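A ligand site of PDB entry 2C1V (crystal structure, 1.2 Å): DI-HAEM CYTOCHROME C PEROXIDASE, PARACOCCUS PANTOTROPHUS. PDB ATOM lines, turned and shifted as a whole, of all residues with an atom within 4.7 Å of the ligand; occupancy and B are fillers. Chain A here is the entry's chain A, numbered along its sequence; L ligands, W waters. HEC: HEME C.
The side-chain amide nitrogen of Gln 118 sits close to a nitrogen (NA) of the ligand (3.0 Å).
Residues that only touch the ligand: Ile 63 (3.4 Å), Ser 64 (3.6 Å), Ser 82 (3.6 Å), Ile 83 (3.7 Å), Gly 84 (3.7 Å), Asn 93 (3.9 Å), Ala 94 (3.8 Å), Pro 95 (3.3 Å), Thr 96 (3.9 Å), Gln 106 (3.6 Å), Leu 115 (3.6 Å), Pro 122 (3.4 Å), Glu 128 (3.6 Å), Met 129 (3.9 Å), Ile 170 (3.5 Å) and Glu 174 (3.5 Å).
25 residues have an atom within 4 Å of the ligand: Ile 63, Ser 64, Cys 65, Cys 68, His 69, Ser 82, Ile 83, Gly 84, Arg 92, Asn 93, Ala 94, Pro 95, Thr 96, Gln 106, Phe 107, Trp 108, Arg 111, Leu 115, Gln 118, Pro 122, Glu 128, Met 129, Ile 170, Glu 174 and Arg 260.
The nearest printed residue that does not touch the ligand is Ala 119 (4.1 Å).
Water W6 bridges NE2 of Gln 118 (3.0 Å) and OE1 of Glu 128 (3.2 Å).
Water W2 bridges O2A of the ligand and O of Thr 96.
Water W3 lies within hydrogen-bond range of the side-chain amide oxygen of Gln 106 (2.7 Å), an oxygen (O2A) of the ligand (2.7 Å), the side-chain amide nitrogen of Asn 103 (2.8 Å) and the guanidinium group of Arg 260 (3.0 Å).
Water W4 lies within hydrogen-bond range of an oxygen (O1A) of the ligand (2.8 Å), the guanidinium group of Arg 260 (3.1 Å) and the backbone NH of Trp 108 (3.3 Å).
N of Cys 65 sits at hydrogen-bond distance from O of Phe 52 (3.2 Å).
ND1 of His 69 sits at hydrogen-bond distance from O of Pro 95, at 3.1 Å.
The backbone carbonyl oxygen (O) of Trp 108 lies within hydrogen-bond range of the backbone NH (N) of Arg 260 (2.9 Å).
The backbone carbonyl oxygen (O) of Gln 106 sits at hydrogen-bond distance from the backbone NH (N) of Arg 111 (3.2 Å).
NE1 of Trp 108 is in hydrogen-bond range of O of Asn 93, 2.9 Å away.
O of Arg 92 is in hydrogen-bond range of N of Ser 82 (3.5 Å).
The backbone NH (N) of Met 129 lies within hydrogen-bond range of the backbone carbonyl oxygen (O) of Pro 122.
The backbone carbonyl oxygen of Val 127 sits close to the backbone NH of Gly 84 (3.5 Å).
The side-chain sulfur (SG) of Cys 65 is bonded to a carbon (CAB) of the ligand (1.8 Å).
CAC of the ligand is covalently linked to SG of Cys 68 (2.0 Å).
NE2 of His 69 is bound to FE of the ligand.
The guanidinium group of Arg 260 is in salt-bridge range of an oxygen (O2A) of the ligand, at 2.7 Å.
N of Phe 107 lies within hydrogen-bond range of O1A of the ligand, at 2.8 Å.
NH1 of Arg 111 is in salt-bridge range of O1D of the ligand, at 2.9 Å.
An oxygen (O2D) of the ligand lies within hydrogen-bond range of the backbone NH (N) of Trp 108 (2.9 Å).
The guanidinium group (NH1) of Arg 92 is in salt-bridge range of an oxygen (O1D) of the ligand (2.9 Å).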
ATOM      1  N   PHE A  52      -0.944  -8.727   1.478  1.00  0.00           N
ATOM      2  CA  PHE A  52       0.349  -8.824   2.147  1.00  0.00           C
ATOM      3  C   PHE A  52       1.046 -10.111   1.768  1.00  0.00           C
ATOM      4  O   PHE A  52       2.301 -10.139   1.716  1.00  0.00           O
ATOM      5  CB  PHE A  52       0.092  -8.717   3.665  1.00  0.00           C
ATOM      6  CG  PHE A  52       1.335  -8.627   4.512  1.00  0.00           C
ATOM      7  CD1 PHE A  52       2.008  -9.774   4.935  1.00  0.00           C
ATOM      8  CD2 PHE A  52       1.827  -7.371   4.919  1.00  0.00           C
ATOM      9  CE1 PHE A  52       3.153  -9.653   5.761  1.00  0.00           C
ATOM     10  CE2 PHE A  52       2.962  -7.255   5.737  1.00  0.00           C
ATOM     11  CZ  PHE A  52       3.610  -8.395   6.125  1.00  0.00           C
ATOM     12  N   ILE A  63       7.759 -12.355  -4.956  1.00  0.00           N
ATOM     13  CA  ILE A  63       8.034 -11.627  -3.717  1.00  0.00           C
ATOM     14  C   ILE A  63       6.764 -10.981  -3.207  1.00  0.00           C
ATOM     15  O   ILE A  63       6.085 -10.257  -3.916  1.00  0.00           O
ATOM     16  CB  ILE A  63       9.104 -10.555  -3.988  1.00  0.00           C
ATOM     17  CG1 ILE A  63      10.401 -11.234  -4.455  1.00  0.00           C
ATOM     18  CG2 ILE A  63       9.333  -9.684  -2.715  1.00  0.00           C
ATOM     19  CD1 ILE A  63      11.451 -10.272  -4.941  1.00  0.00           C
ATOM     20  N   SER A  64       6.432 -11.266  -1.948  1.00  0.00           N
ATOM     21  CA  SER A  64       5.326 -10.599  -1.255  1.00  0.00           C
ATOM     22  C   SER A  64       5.897  -9.819  -0.073  1.00  0.00           C
ATOM     23  O   SER A  64       7.091  -9.920   0.265  1.00  0.00           O
ATOM     24  CB  SER A  64       4.298 -11.601  -0.741  1.00  0.00           C
ATOM     25  OG  SER A  64       4.852 -12.351   0.346  1.00  0.00           O
ATOM     26  N   CYS A  65       5.057  -9.063   0.634  1.00  0.00           N
ATOM     27  CA  CYS A  65       5.534  -8.437   1.867  1.00  0.00           C
ATOM     28  C   CYS A  65       6.069  -9.475   2.836  1.00  0.00           C
ATOM     29  O   CYS A  65       7.059  -9.242   3.532  1.00  0.00           O
ATOM     30  CB  CYS A  65       4.397  -7.689   2.568  1.00  0.00           C
ATOM     31  SG  CYS A  65       3.437  -6.564   1.503  1.00  0.00           S
ATOM     32  N   CYS A  68       9.912 -10.628   3.031  1.00  0.00           N
ATOM     33  CA  CYS A  68      10.874  -9.908   3.824  1.00  0.00           C
ATOM     34  C   CYS A  68      10.426  -9.641   5.250  1.00  0.00           C
ATOM     35  O   CYS A  68      11.270  -9.271   6.110  1.00  0.00           O
ATOM     36  CB  CYS A  68      11.249  -8.595   3.172  1.00  0.00           C
ATOM     37  SG  CYS A  68      11.999  -8.902   1.556  1.00  0.00           S
ATOM     38  N   HIS A  69       9.138  -9.773   5.524  1.00  0.00           N
ATOM     39  CA  HIS A  69       8.584  -9.523   6.840  1.00  0.00           C
ATOM     40  C   HIS A  69       7.894 -10.780   7.312  1.00  0.00           C
ATOM     41  O   HIS A  69       6.651 -10.836   7.420  1.00  0.00           O
ATOM     42  CB  HIS A  69       7.654  -8.307   6.820  1.00  0.00           C
ATOM     43  CG  HIS A  69       8.338  -7.056   6.398  1.00  0.00           C
ATOM     44  ND1 HIS A  69       9.152  -6.326   7.238  1.00  0.00           N
ATOM     45  CD2 HIS A  69       8.313  -6.389   5.227  1.00  0.00           C
ATOM     46  CE1 HIS A  69       9.605  -5.261   6.604  1.00  0.00           C
ATOM     47  NE2 HIS A  69       9.112  -5.276   5.368  1.00  0.00           N
ATOM     48  N   SER A  82      18.067  -6.712   3.154  1.00  0.00           N
ATOM     49  CA  SER A  82      17.123  -7.512   2.381  1.00  0.00           C
ATOM     50  C   SER A  82      17.581  -7.813   0.985  1.00  0.00           C
ATOM     51  O   SER A  82      18.341  -7.039   0.345  1.00  0.00           O
ATOM     52  CB  SER A  82      15.764  -6.828   2.360  1.00  0.00           C
ATOM     53  OG  SER A  82      15.191  -6.759   3.665  1.00  0.00           O
ATOM     54  N   ILE A  83      17.085  -8.908   0.456  1.00  0.00           N
ATOM     55  CA  ILE A  83      17.371  -9.391  -0.893  1.00  0.00           C
ATOM     56  C   ILE A  83      16.027  -9.486  -1.612  1.00  0.00           C
ATOM     57  O   ILE A  83      15.127 -10.204  -1.140  1.00  0.00           O
ATOM     58  CB  ILE A  83      17.989 -10.791  -0.797  1.00  0.00           C
ATOM     59  CG1 ILE A  83      19.251 -10.791   0.048  1.00  0.00           C
ATOM     60  CG2 ILE A  83      18.202 -11.364  -2.198  1.00  0.00           C
ATOM     61  CD1 ILE A  83      20.367 -10.066  -0.510  1.00  0.00           C
ATOM     62  N   GLY A  84      15.874  -8.754  -2.720  1.00  0.00           N
ATOM     63  CA  GLY A  84      14.584  -8.632  -3.406  1.00  0.00           C
ATOM     64  C   GLY A  84      14.687  -9.051  -4.843  1.00  0.00           C
ATOM     65  O   GLY A  84      15.367 -10.030  -5.180  1.00  0.00           O
ATOM     66  N   ARG A  92      19.725  -1.589   3.725  1.00  0.00           N
ATOM     67  CA  ARG A  92      19.328  -1.583   5.124  1.00  0.00           C
ATOM     68  C   ARG A  92      18.675  -2.885   5.558  1.00  0.00           C
ATOM     69  O   ARG A  92      18.063  -3.598   4.749  1.00  0.00           O
ATOM     70  CB  ARG A  92      18.414  -0.401   5.443  1.00  0.00           C
ATOM     71  CG  ARG A  92      19.092   0.957   5.385  1.00  0.00           C
ATOM     72  CD  ARG A  92      18.101   2.073   5.657  1.00  0.00           C
ATOM     73  NE  ARG A  92      18.751   3.381   5.641  1.00  0.00           N
ATOM     74  CZ  ARG A  92      18.075   4.513   5.495  1.00  0.00           C
ATOM     75  NH1 ARG A  92      16.759   4.508   5.333  1.00  0.00           N
ATOM     76  NH2 ARG A  92      18.729   5.677   5.517  1.00  0.00           N
ATOM     77  N   ASN A  93      18.771  -3.146   6.861  1.00  0.00           N
ATOM     78  CA  ASN A  93      18.116  -4.271   7.515  1.00  0.00           C
ATOM     79  C   ASN A  93      16.607  -4.068   7.564  1.00  0.00           C
ATOM     80  O   ASN A  93      16.138  -2.974   7.863  1.00  0.00           O
ATOM     81  CB  ASN A  93      18.725  -4.313   8.926  1.00  0.00           C
ATOM     82  CG  ASN A  93      18.273  -5.523   9.727  1.00  0.00           C
ATOM     83  OD1 ASN A  93      17.422  -5.421  10.623  1.00  0.00           O
ATOM     84  ND2 ASN A  93      18.802  -6.662   9.384  1.00  0.00           N
ATOM     85  N   ALA A  94      15.855  -5.122   7.276  1.00  0.00           N
ATOM     86  CA  ALA A  94      14.395  -5.012   7.322  1.00  0.00           C
ATOM     87  C   ALA A  94      13.901  -4.987   8.769  1.00  0.00           C
ATOM     88  O   ALA A  94      14.151  -5.932   9.520  1.00  0.00           O
ATOM     89  CB  ALA A  94      13.747  -6.157   6.549  1.00  0.00           C
ATOM     90  N   PRO A  95      13.209  -3.933   9.170  1.00  0.00           N
ATOM     91  CA  PRO A  95      12.585  -3.848  10.521  1.00  0.00           C
ATOM     92  C   PRO A  95      11.274  -4.597  10.502  1.00  0.00           C
ATOM     93  O   PRO A  95      10.664  -4.873   9.471  1.00  0.00           O
ATOM     94  CB  PRO A  95      12.323  -2.326  10.703  1.00  0.00           C
ATOM     95  CG  PRO A  95      12.046  -1.886   9.233  1.00  0.00           C
ATOM     96  CD  PRO A  95      12.919  -2.719   8.361  1.00  0.00           C
ATOM     97  N   THR A  96      10.775  -4.931  11.688  1.00  0.00           N
ATOM     98  CA  THR A  96       9.518  -5.628  11.793  1.00  0.00           C
ATOM     99  C   THR A  96       8.321  -4.738  11.499  1.00  0.00           C
ATOM    100  O   THR A  96       8.300  -3.557  11.818  1.00  0.00           O
ATOM    101  CB  THR A  96       9.391  -6.251  13.211  1.00  0.00           C
ATOM    102  OG1 THR A  96       8.205  -7.029  13.250  1.00  0.00           O
ATOM    103  CG2 THR A  96       9.273  -5.226  14.357  1.00  0.00           C
ATOM    104  N   MET A  97       7.287  -5.323  10.918  1.00  0.00           N
ATOM    105  CA  MET A  97       5.986  -4.660  10.857  1.00  0.00           C
ATOM    106  C   MET A  97       5.181  -4.837  12.161  1.00  0.00           C
ATOM    107  O   MET A  97       4.168  -4.150  12.346  1.00  0.00           O
ATOM    108  CB  MET A  97       5.138  -5.039   9.615  1.00  0.00           C
ATOM    109  CG  MET A  97       4.373  -6.329   9.728  1.00  0.00           C
ATOM    110  SD  MET A  97       5.510  -7.710   9.695  1.00  0.00           S
ATOM    111  CE  MET A  97       4.439  -9.165   9.701  1.00  0.00           C
ATOM    112  N   ALA A 100       4.377  -1.799  14.288  1.00  0.00           N
ATOM    113  CA  ALA A 100       4.817  -0.628  13.551  1.00  0.00           C
ATOM    114  C   ALA A 100       3.773   0.480  13.569  1.00  0.00           C
ATOM    115  O   ALA A 100       4.110   1.665  13.483  1.00  0.00           O
ATOM    116  CB  ALA A 100       5.172  -1.012  12.089  1.00  0.00           C
ATOM    117  N   ASN A 103       4.563   3.508  15.854  1.00  0.00           N
ATOM    118  CA  ASN A 103       5.724   4.392  15.676  1.00  0.00           C
ATOM    119  C   ASN A 103       5.310   5.708  15.031  1.00  0.00           C
ATOM    120  O   ASN A 103       4.332   5.782  14.297  1.00  0.00           O
ATOM    121  CB  ASN A 103       6.809   3.641  14.947  1.00  0.00           C
ATOM    122  CG  ASN A 103       7.267   2.431  15.762  1.00  0.00           C
ATOM    123  OD1 ASN A 103       7.424   2.552  16.984  1.00  0.00           O
ATOM    124  ND2 ASN A 103       7.338   1.266  15.152  1.00  0.00           N
ATOM    125  N   GLN A 106       7.665   5.952   9.793  1.00  0.00           N
ATOM    126  CA  GLN A 106       8.116   4.648   9.319  1.00  0.00           C
ATOM    127  C   GLN A 106       9.430   4.785   8.564  1.00  0.00           C
ATOM    128  O   GLN A 106       9.720   5.845   7.980  1.00  0.00           O
ATOM    129  CB  GLN A 106       7.051   4.054   8.370  1.00  0.00           C
ATOM    130  CG  GLN A 106       5.660   3.978   9.007  1.00  0.00           C
ATOM    131  CD  GLN A 106       5.610   3.034  10.157  1.00  0.00           C
ATOM    132  OE1 GLN A 106       6.232   1.974  10.121  1.00  0.00           O
ATOM    133  NE2 GLN A 106       4.839   3.371  11.167  1.00  0.00           N
ATOM    134  N   PHE A 107      10.140   3.650   8.500  1.00  0.00           N
ATOM    135  CA  PHE A 107      11.510   3.503   7.966  1.00  0.00           C
ATOM    136  C   PHE A 107      12.557   3.983   8.966  1.00  0.00           C
ATOM    137  O   PHE A 107      12.272   4.781   9.885  1.00  0.00           O
ATOM    138  CB  PHE A 107      11.705   4.205   6.612  1.00  0.00           C
ATOM    139  CG  PHE A 107      10.871   3.650   5.489  1.00  0.00           C
ATOM    140  CD1 PHE A 107      11.036   2.339   5.044  1.00  0.00           C
ATOM    141  CD2 PHE A 107       9.987   4.484   4.808  1.00  0.00           C
ATOM    142  CE1 PHE A 107      10.306   1.862   3.949  1.00  0.00           C
ATOM    143  CE2 PHE A 107       9.281   4.008   3.705  1.00  0.00           C
ATOM    144  CZ  PHE A 107       9.457   2.701   3.269  1.00  0.00           C
ATOM    145  N   TRP A 108      13.788   3.551   8.768  1.00  0.00           N
ATOM    146  CA  TRP A 108      14.875   3.893   9.664  1.00  0.00           C
ATOM    147  C   TRP A 108      15.161   5.401   9.695  1.00  0.00           C
ATOM    148  O   TRP A 108      15.791   5.861  10.659  1.00  0.00           O
ATOM    149  CB  TRP A 108      16.154   3.173   9.219  1.00  0.00           C
ATOM    150  CG  TRP A 108      16.235   1.705   9.573  1.00  0.00           C
ATOM    151  CD1 TRP A 108      15.987   0.668   8.708  1.00  0.00           C
ATOM    152  CD2 TRP A 108      16.614   1.116  10.820  1.00  0.00           C
ATOM    153  NE1 TRP A 108      16.171  -0.521   9.358  1.00  0.00           N
ATOM    154  CE2 TRP A 108      16.566  -0.282  10.642  1.00  0.00           C
ATOM    155  CE3 TRP A 108      17.014   1.598  12.064  1.00  0.00           C
ATOM    156  CZ2 TRP A 108      16.865  -1.196  11.651  1.00  0.00           C
ATOM    157  CZ3 TRP A 108      17.331   0.676  13.063  1.00  0.00           C
ATOM    158  CH2 TRP A 108      17.247  -0.674  12.844  1.00  0.00           C
ATOM    159  N   ARG A 111      11.060   8.501   6.798  1.00  0.00           N
ATOM    160  CA  ARG A 111      10.619   9.216   5.589  1.00  0.00           C
ATOM    161  C   ARG A 111       9.174   8.984   5.162  1.00  0.00           C
ATOM    162  O   ARG A 111       8.695   9.715   4.287  1.00  0.00           O
ATOM    163  CB  ARG A 111      11.570   8.949   4.446  1.00  0.00           C
ATOM    164  CG  ARG A 111      11.461   7.574   3.870  1.00  0.00           C
ATOM    165  CD  ARG A 111      12.531   7.363   2.773  1.00  0.00           C
ATOM    166  NE  ARG A 111      12.492   6.028   2.218  1.00  0.00           N
ATOM    167  CZ  ARG A 111      13.063   4.956   2.763  1.00  0.00           C
ATOM    168  NH1 ARG A 111      13.721   5.052   3.904  1.00  0.00           N
ATOM    169  NH2 ARG A 111      12.931   3.782   2.145  1.00  0.00           N
ATOM    170  N   LEU A 115       1.617   3.875   7.827  1.00  0.00           N
ATOM    171  CA  LEU A 115       1.711   2.602   7.117  1.00  0.00           C
ATOM    172  C   LEU A 115       1.195   2.611   5.685  1.00  0.00           C
ATOM    173  O   LEU A 115       1.704   1.902   4.839  1.00  0.00           O
ATOM    174  CB  LEU A 115       1.060   1.473   7.907  1.00  0.00           C
ATOM    175  CG  LEU A 115       1.648   1.228   9.310  1.00  0.00           C
ATOM    176  CD1 LEU A 115       0.804   0.183  10.051  1.00  0.00           C
ATOM    177  CD2 LEU A 115       3.052   0.649   9.184  1.00  0.00           C
ATOM    178  N   GLN A 118       3.914   4.238   3.727  1.00  0.00           N
ATOM    179  CA  GLN A 118       5.065   3.311   3.662  1.00  0.00           C
ATOM    180  C   GLN A 118       4.866   2.255   2.577  1.00  0.00           C
ATOM    181  O   GLN A 118       5.822   1.931   1.862  1.00  0.00           O
ATOM    182  CB  GLN A 118       5.227   2.645   5.011  1.00  0.00           C
ATOM    183  CG  GLN A 118       6.484   1.767   5.127  1.00  0.00           C
ATOM    184  CD  GLN A 118       6.389   0.438   4.380  1.00  0.00           C
ATOM    185  OE1 GLN A 118       5.302  -0.116   4.222  1.00  0.00           O
ATOM    186  NE2 GLN A 118       7.519  -0.056   3.862  1.00  0.00           N
ATOM    187  N   ALA A 119       3.647   1.717   2.452  1.00  0.00           N
ATOM    188  CA  ALA A 119       3.424   0.466   1.698  1.00  0.00           C
ATOM    189  C   ALA A 119       3.661   0.712   0.225  1.00  0.00           C
ATOM    190  O   ALA A 119       3.962  -0.211  -0.545  1.00  0.00           O
ATOM    191  CB  ALA A 119       1.983  -0.033   1.920  1.00  0.00           C
ATOM    192  N   PRO A 122       7.929  -0.313  -1.042  1.00  0.00           N
ATOM    193  CA  PRO A 122       8.416  -1.630  -1.483  1.00  0.00           C
ATOM    194  C   PRO A 122       7.853  -2.059  -2.808  1.00  0.00           C
ATOM    195  O   PRO A 122       8.543  -2.700  -3.601  1.00  0.00           O
ATOM    196  CB  PRO A 122       7.995  -2.586  -0.347  1.00  0.00           C
ATOM    197  CG  PRO A 122       6.942  -1.822   0.407  1.00  0.00           C
ATOM    198  CD  PRO A 122       7.351  -0.375   0.303  1.00  0.00           C
ATOM    199  N   VAL A 123       6.601  -1.704  -3.070  1.00  0.00           N
ATOM    200  CA  VAL A 123       5.984  -2.094  -4.331  1.00  0.00           C
ATOM    201  C   VAL A 123       6.786  -1.565  -5.498  1.00  0.00           C
ATOM    202  O   VAL A 123       6.952  -2.263  -6.513  1.00  0.00           O
ATOM    203  CB  VAL A 123       4.536  -1.581  -4.411  1.00  0.00           C
ATOM    204  CG1 VAL A 123       3.985  -1.771  -5.837  1.00  0.00           C
ATOM    205  CG2 VAL A 123       3.669  -2.278  -3.390  1.00  0.00           C
ATOM    206  N   VAL A 127      14.907  -2.697  -5.903  1.00  0.00           N
ATOM    207  CA  VAL A 127      15.562  -3.773  -5.128  1.00  0.00           C
ATOM    208  C   VAL A 127      14.593  -4.552  -4.250  1.00  0.00           C
ATOM    209  O   VAL A 127      15.017  -5.512  -3.589  1.00  0.00           O
ATOM    210  CB  VAL A 127      16.750  -3.249  -4.272  1.00  0.00           C
ATOM    211  CG1 VAL A 127      17.806  -2.581  -5.157  1.00  0.00           C
ATOM    212  CG2 VAL A 127      16.273  -2.324  -3.134  1.00  0.00           C
ATOM    213  N   GLU A 128      13.301  -4.159  -4.225  1.00  0.00           N
ATOM    214  CA  GLU A 128      12.303  -4.881  -3.451  1.00  0.00           C
ATOM    215  C   GLU A 128      11.335  -5.544  -4.421  1.00  0.00           C
ATOM    216  O   GLU A 128      11.715  -6.549  -5.026  1.00  0.00           O
ATOM    217  CB  GLU A 128      11.682  -3.955  -2.419  1.00  0.00           C
ATOM    218  CG  GLU A 128      12.777  -3.479  -1.471  1.00  0.00           C
ATOM    219  CD  GLU A 128      12.290  -2.731  -0.272  1.00  0.00           C
ATOM    220  OE1 GLU A 128      11.053  -2.691  -0.024  1.00  0.00           O
ATOM    221  OE2 GLU A 128      13.153  -2.240   0.495  1.00  0.00           O
ATOM    222  N   MET A 129      10.121  -5.017  -4.601  1.00  0.00           N
ATOM    223  CA  MET A 129       9.135  -5.730  -5.429  1.00  0.00           C
ATOM    224  C   MET A 129       9.203  -5.327  -6.909  1.00  0.00           C
ATOM    225  O   MET A 129       8.628  -6.016  -7.772  1.00  0.00           O
ATOM    226  CB  MET A 129       7.730  -5.545  -4.880  1.00  0.00           C
ATOM    227  CG  MET A 129       7.636  -6.114  -3.475  1.00  0.00           C
ATOM    228  SD  MET A 129       6.146  -5.727  -2.543  1.00  0.00           S
ATOM    229  CE  MET A 129       4.956  -6.790  -3.376  1.00  0.00           C
ATOM    230  N   PHE A 166      -5.222  -0.024  -2.111  1.00  0.00           N
ATOM    231  CA  PHE A 166      -4.284  -1.132  -1.834  1.00  0.00           C
ATOM    232  C   PHE A 166      -3.480  -0.816  -0.560  1.00  0.00           C
ATOM    233  O   PHE A 166      -3.411  -1.630   0.354  1.00  0.00           O
ATOM    234  CB  PHE A 166      -3.396  -1.317  -3.061  1.00  0.00           C
ATOM    235  CG  PHE A 166      -2.171  -2.155  -2.823  1.00  0.00           C
ATOM    236  CD1 PHE A 166      -0.984  -1.564  -2.393  1.00  0.00           C
ATOM    237  CD2 PHE A 166      -2.188  -3.519  -3.089  1.00  0.00           C
ATOM    238  CE1 PHE A 166       0.185  -2.330  -2.206  1.00  0.00           C
ATOM    239  CE2 PHE A 166      -1.011  -4.297  -2.918  1.00  0.00           C
ATOM    240  CZ  PHE A 166       0.156  -3.691  -2.456  1.00  0.00           C
ATOM    241  N   ILE A 170      -3.639  -2.658   3.237  1.00  0.00           N
ATOM    242  CA  ILE A 170      -2.440  -3.187   3.920  1.00  0.00           C
ATOM    243  C   ILE A 170      -2.250  -2.530   5.291  1.00  0.00           C
ATOM    244  O   ILE A 170      -1.983  -3.227   6.260  1.00  0.00           O
ATOM    245  CB  ILE A 170      -1.207  -2.993   3.018  1.00  0.00           C
ATOM    246  CG1 ILE A 170      -1.346  -3.933   1.811  1.00  0.00           C
ATOM    247  CG2 ILE A 170       0.087  -3.240   3.818  1.00  0.00           C
ATOM    248  CD1 ILE A 170      -0.229  -3.892   0.824  1.00  0.00           C
ATOM    249  N   GLU A 174      -2.015  -4.442   8.863  1.00  0.00           N
ATOM    250  CA  GLU A 174      -0.814  -4.305   9.691  1.00  0.00           C
ATOM    251  C   GLU A 174      -1.160  -3.691  11.051  1.00  0.00           C
ATOM    252  O   GLU A 174      -0.499  -4.023  12.034  1.00  0.00           O
ATOM    253  CB  GLU A 174       0.242  -3.468   9.002  1.00  0.00           C
ATOM    254  CG  GLU A 174       0.885  -4.174   7.817  1.00  0.00           C
ATOM    255  CD  GLU A 174       1.928  -3.263   7.193  1.00  0.00           C
ATOM    256  OE1 GLU A 174       1.548  -2.121   6.788  1.00  0.00           O
ATOM    257  OE2 GLU A 174       3.113  -3.636   7.114  1.00  0.00           O
ATOM    258  N   ARG A 260      16.046   7.047  13.263  1.00  0.00           N
ATOM    259  CA  ARG A 260      14.974   6.829  14.223  1.00  0.00           C
ATOM    260  C   ARG A 260      15.413   5.864  15.308  1.00  0.00           C
ATOM    261  O   ARG A 260      16.029   4.843  15.007  1.00  0.00           O
ATOM    262  CB  ARG A 260      13.764   6.270  13.490  1.00  0.00           C
ATOM    263  CG  ARG A 260      12.529   6.138  14.375  1.00  0.00           C
ATOM    264  CD  ARG A 260      11.384   5.413  13.683  1.00  0.00           C
ATOM    265  NE  ARG A 260      11.746   3.989  13.626  1.00  0.00           N
ATOM    266  CZ  ARG A 260      10.903   3.050  13.208  1.00  0.00           C
ATOM    267  NH1 ARG A 260       9.668   3.358  12.786  1.00  0.00           N
ATOM    268  NH2 ARG A 260      11.295   1.771  13.206  1.00  0.00           N
HETATM  269 FE   HEC L   1       9.181  -3.739   4.026  1.00  0.00          FE
HETATM  270  CHA HEC L   1      10.547  -1.316   5.957  1.00  0.00           C
HETATM  271  CHB HEC L   1       6.128  -3.061   5.297  1.00  0.00           C
HETATM  272  CHC HEC L   1       7.734  -5.426   1.455  1.00  0.00           C
HETATM  273  CHD HEC L   1      12.214  -4.837   3.116  1.00  0.00           C
HETATM  274  NA  HEC L   1       8.510  -2.452   5.404  1.00  0.00           N
HETATM  275  C1A HEC L   1       9.228  -1.578   6.156  1.00  0.00           C
HETATM  276  C2A HEC L   1       8.356  -0.955   7.120  1.00  0.00           C
HETATM  277  C3A HEC L   1       7.120  -1.491   6.966  1.00  0.00           C
HETATM  278  C4A HEC L   1       7.210  -2.406   5.862  1.00  0.00           C
HETATM  279  CMA HEC L   1       5.838  -1.147   7.738  1.00  0.00           C
HETATM  280  CAA HEC L   1       8.810   0.087   8.128  1.00  0.00           C
HETATM  281  CBA HEC L   1       8.884  -0.432   9.541  1.00  0.00           C
HETATM  282  CGA HEC L   1       9.810   0.356  10.434  1.00  0.00           C
HETATM  283  O1A HEC L   1      10.573   1.252   9.924  1.00  0.00           O
HETATM  284  O2A HEC L   1       9.813   0.064  11.667  1.00  0.00           O
HETATM  285  NB  HEC L   1       7.291  -4.100   3.421  1.00  0.00           N
HETATM  286  C1B HEC L   1       6.156  -3.705   4.064  1.00  0.00           C
HETATM  287  C2B HEC L   1       5.031  -4.034   3.200  1.00  0.00           C
HETATM  288  C3B HEC L   1       5.484  -4.739   2.175  1.00  0.00           C
HETATM  289  C4B HEC L   1       6.910  -4.759   2.289  1.00  0.00           C
HETATM  290  CMB HEC L   1       3.569  -3.769   3.656  1.00  0.00           C
HETATM  291  CAB HEC L   1       4.652  -5.343   0.999  1.00  0.00           C
HETATM  292  CBB HEC L   1       3.929  -4.199   0.231  1.00  0.00           C
HETATM  293  NC  HEC L   1       9.862  -4.888   2.543  1.00  0.00           N
HETATM  294  C1C HEC L   1       9.101  -5.568   1.590  1.00  0.00           C
HETATM  295  C2C HEC L   1       9.962  -6.412   0.816  1.00  0.00           C
HETATM  296  C3C HEC L   1      11.198  -6.265   1.300  1.00  0.00           C
HETATM  297  C4C HEC L   1      11.157  -5.324   2.373  1.00  0.00           C
HETATM  298  CMC HEC L   1       9.469  -7.337  -0.292  1.00  0.00           C
HETATM  299  CAC HEC L   1      12.425  -7.081   0.968  1.00  0.00           C
HETATM  300  CBC HEC L   1      12.946  -7.255  -0.421  1.00  0.00           C
HETATM  301  ND  HEC L   1      11.053  -3.159   4.470  1.00  0.00           N
HETATM  302  C1D HEC L   1      12.181  -3.713   3.913  1.00  0.00           C
HETATM  303  C2D HEC L   1      13.335  -2.979   4.333  1.00  0.00           C
HETATM  304  C3D HEC L   1      12.826  -1.875   5.138  1.00  0.00           C
HETATM  305  C4D HEC L   1      11.409  -2.055   5.224  1.00  0.00           C
HETATM  306  CMD HEC L   1      14.800  -3.240   3.971  1.00  0.00           C
HETATM  307  CAD HEC L   1      13.692  -0.771   5.772  1.00  0.00           C
HETATM  308  CBD HEC L   1      14.006   0.312   4.675  1.00  0.00           C
HETATM  309  CGD HEC L   1      14.423   1.661   5.222  1.00  0.00           C
HETATM  310  O1D HEC L   1      14.911   2.481   4.399  1.00  0.00           O
HETATM  311  O2D HEC L   1      14.271   1.932   6.417  1.00  0.00           O
HETATM  312  O   HOH W   1      11.558  -0.754   2.184  1.00  0.00           O
HETATM  313  O   HOH W   2       9.639  -1.882  13.431  1.00  0.00           O
HETATM  314  O   HOH W   3       7.522   1.296  12.380  1.00  0.00           O
HETATM  315  O   HOH W   4      13.224   1.057  10.830  1.00  0.00           O
HETATM  316  O   HOH W   5      17.599  -2.750   2.234  1.00  0.00           O
HETATM  317  O   HOH W   6       9.308  -2.157   2.641  1.00  0.00           O
HETATM  318  O   HOH W   7      16.106   1.582   2.160  1.00  0.00           O
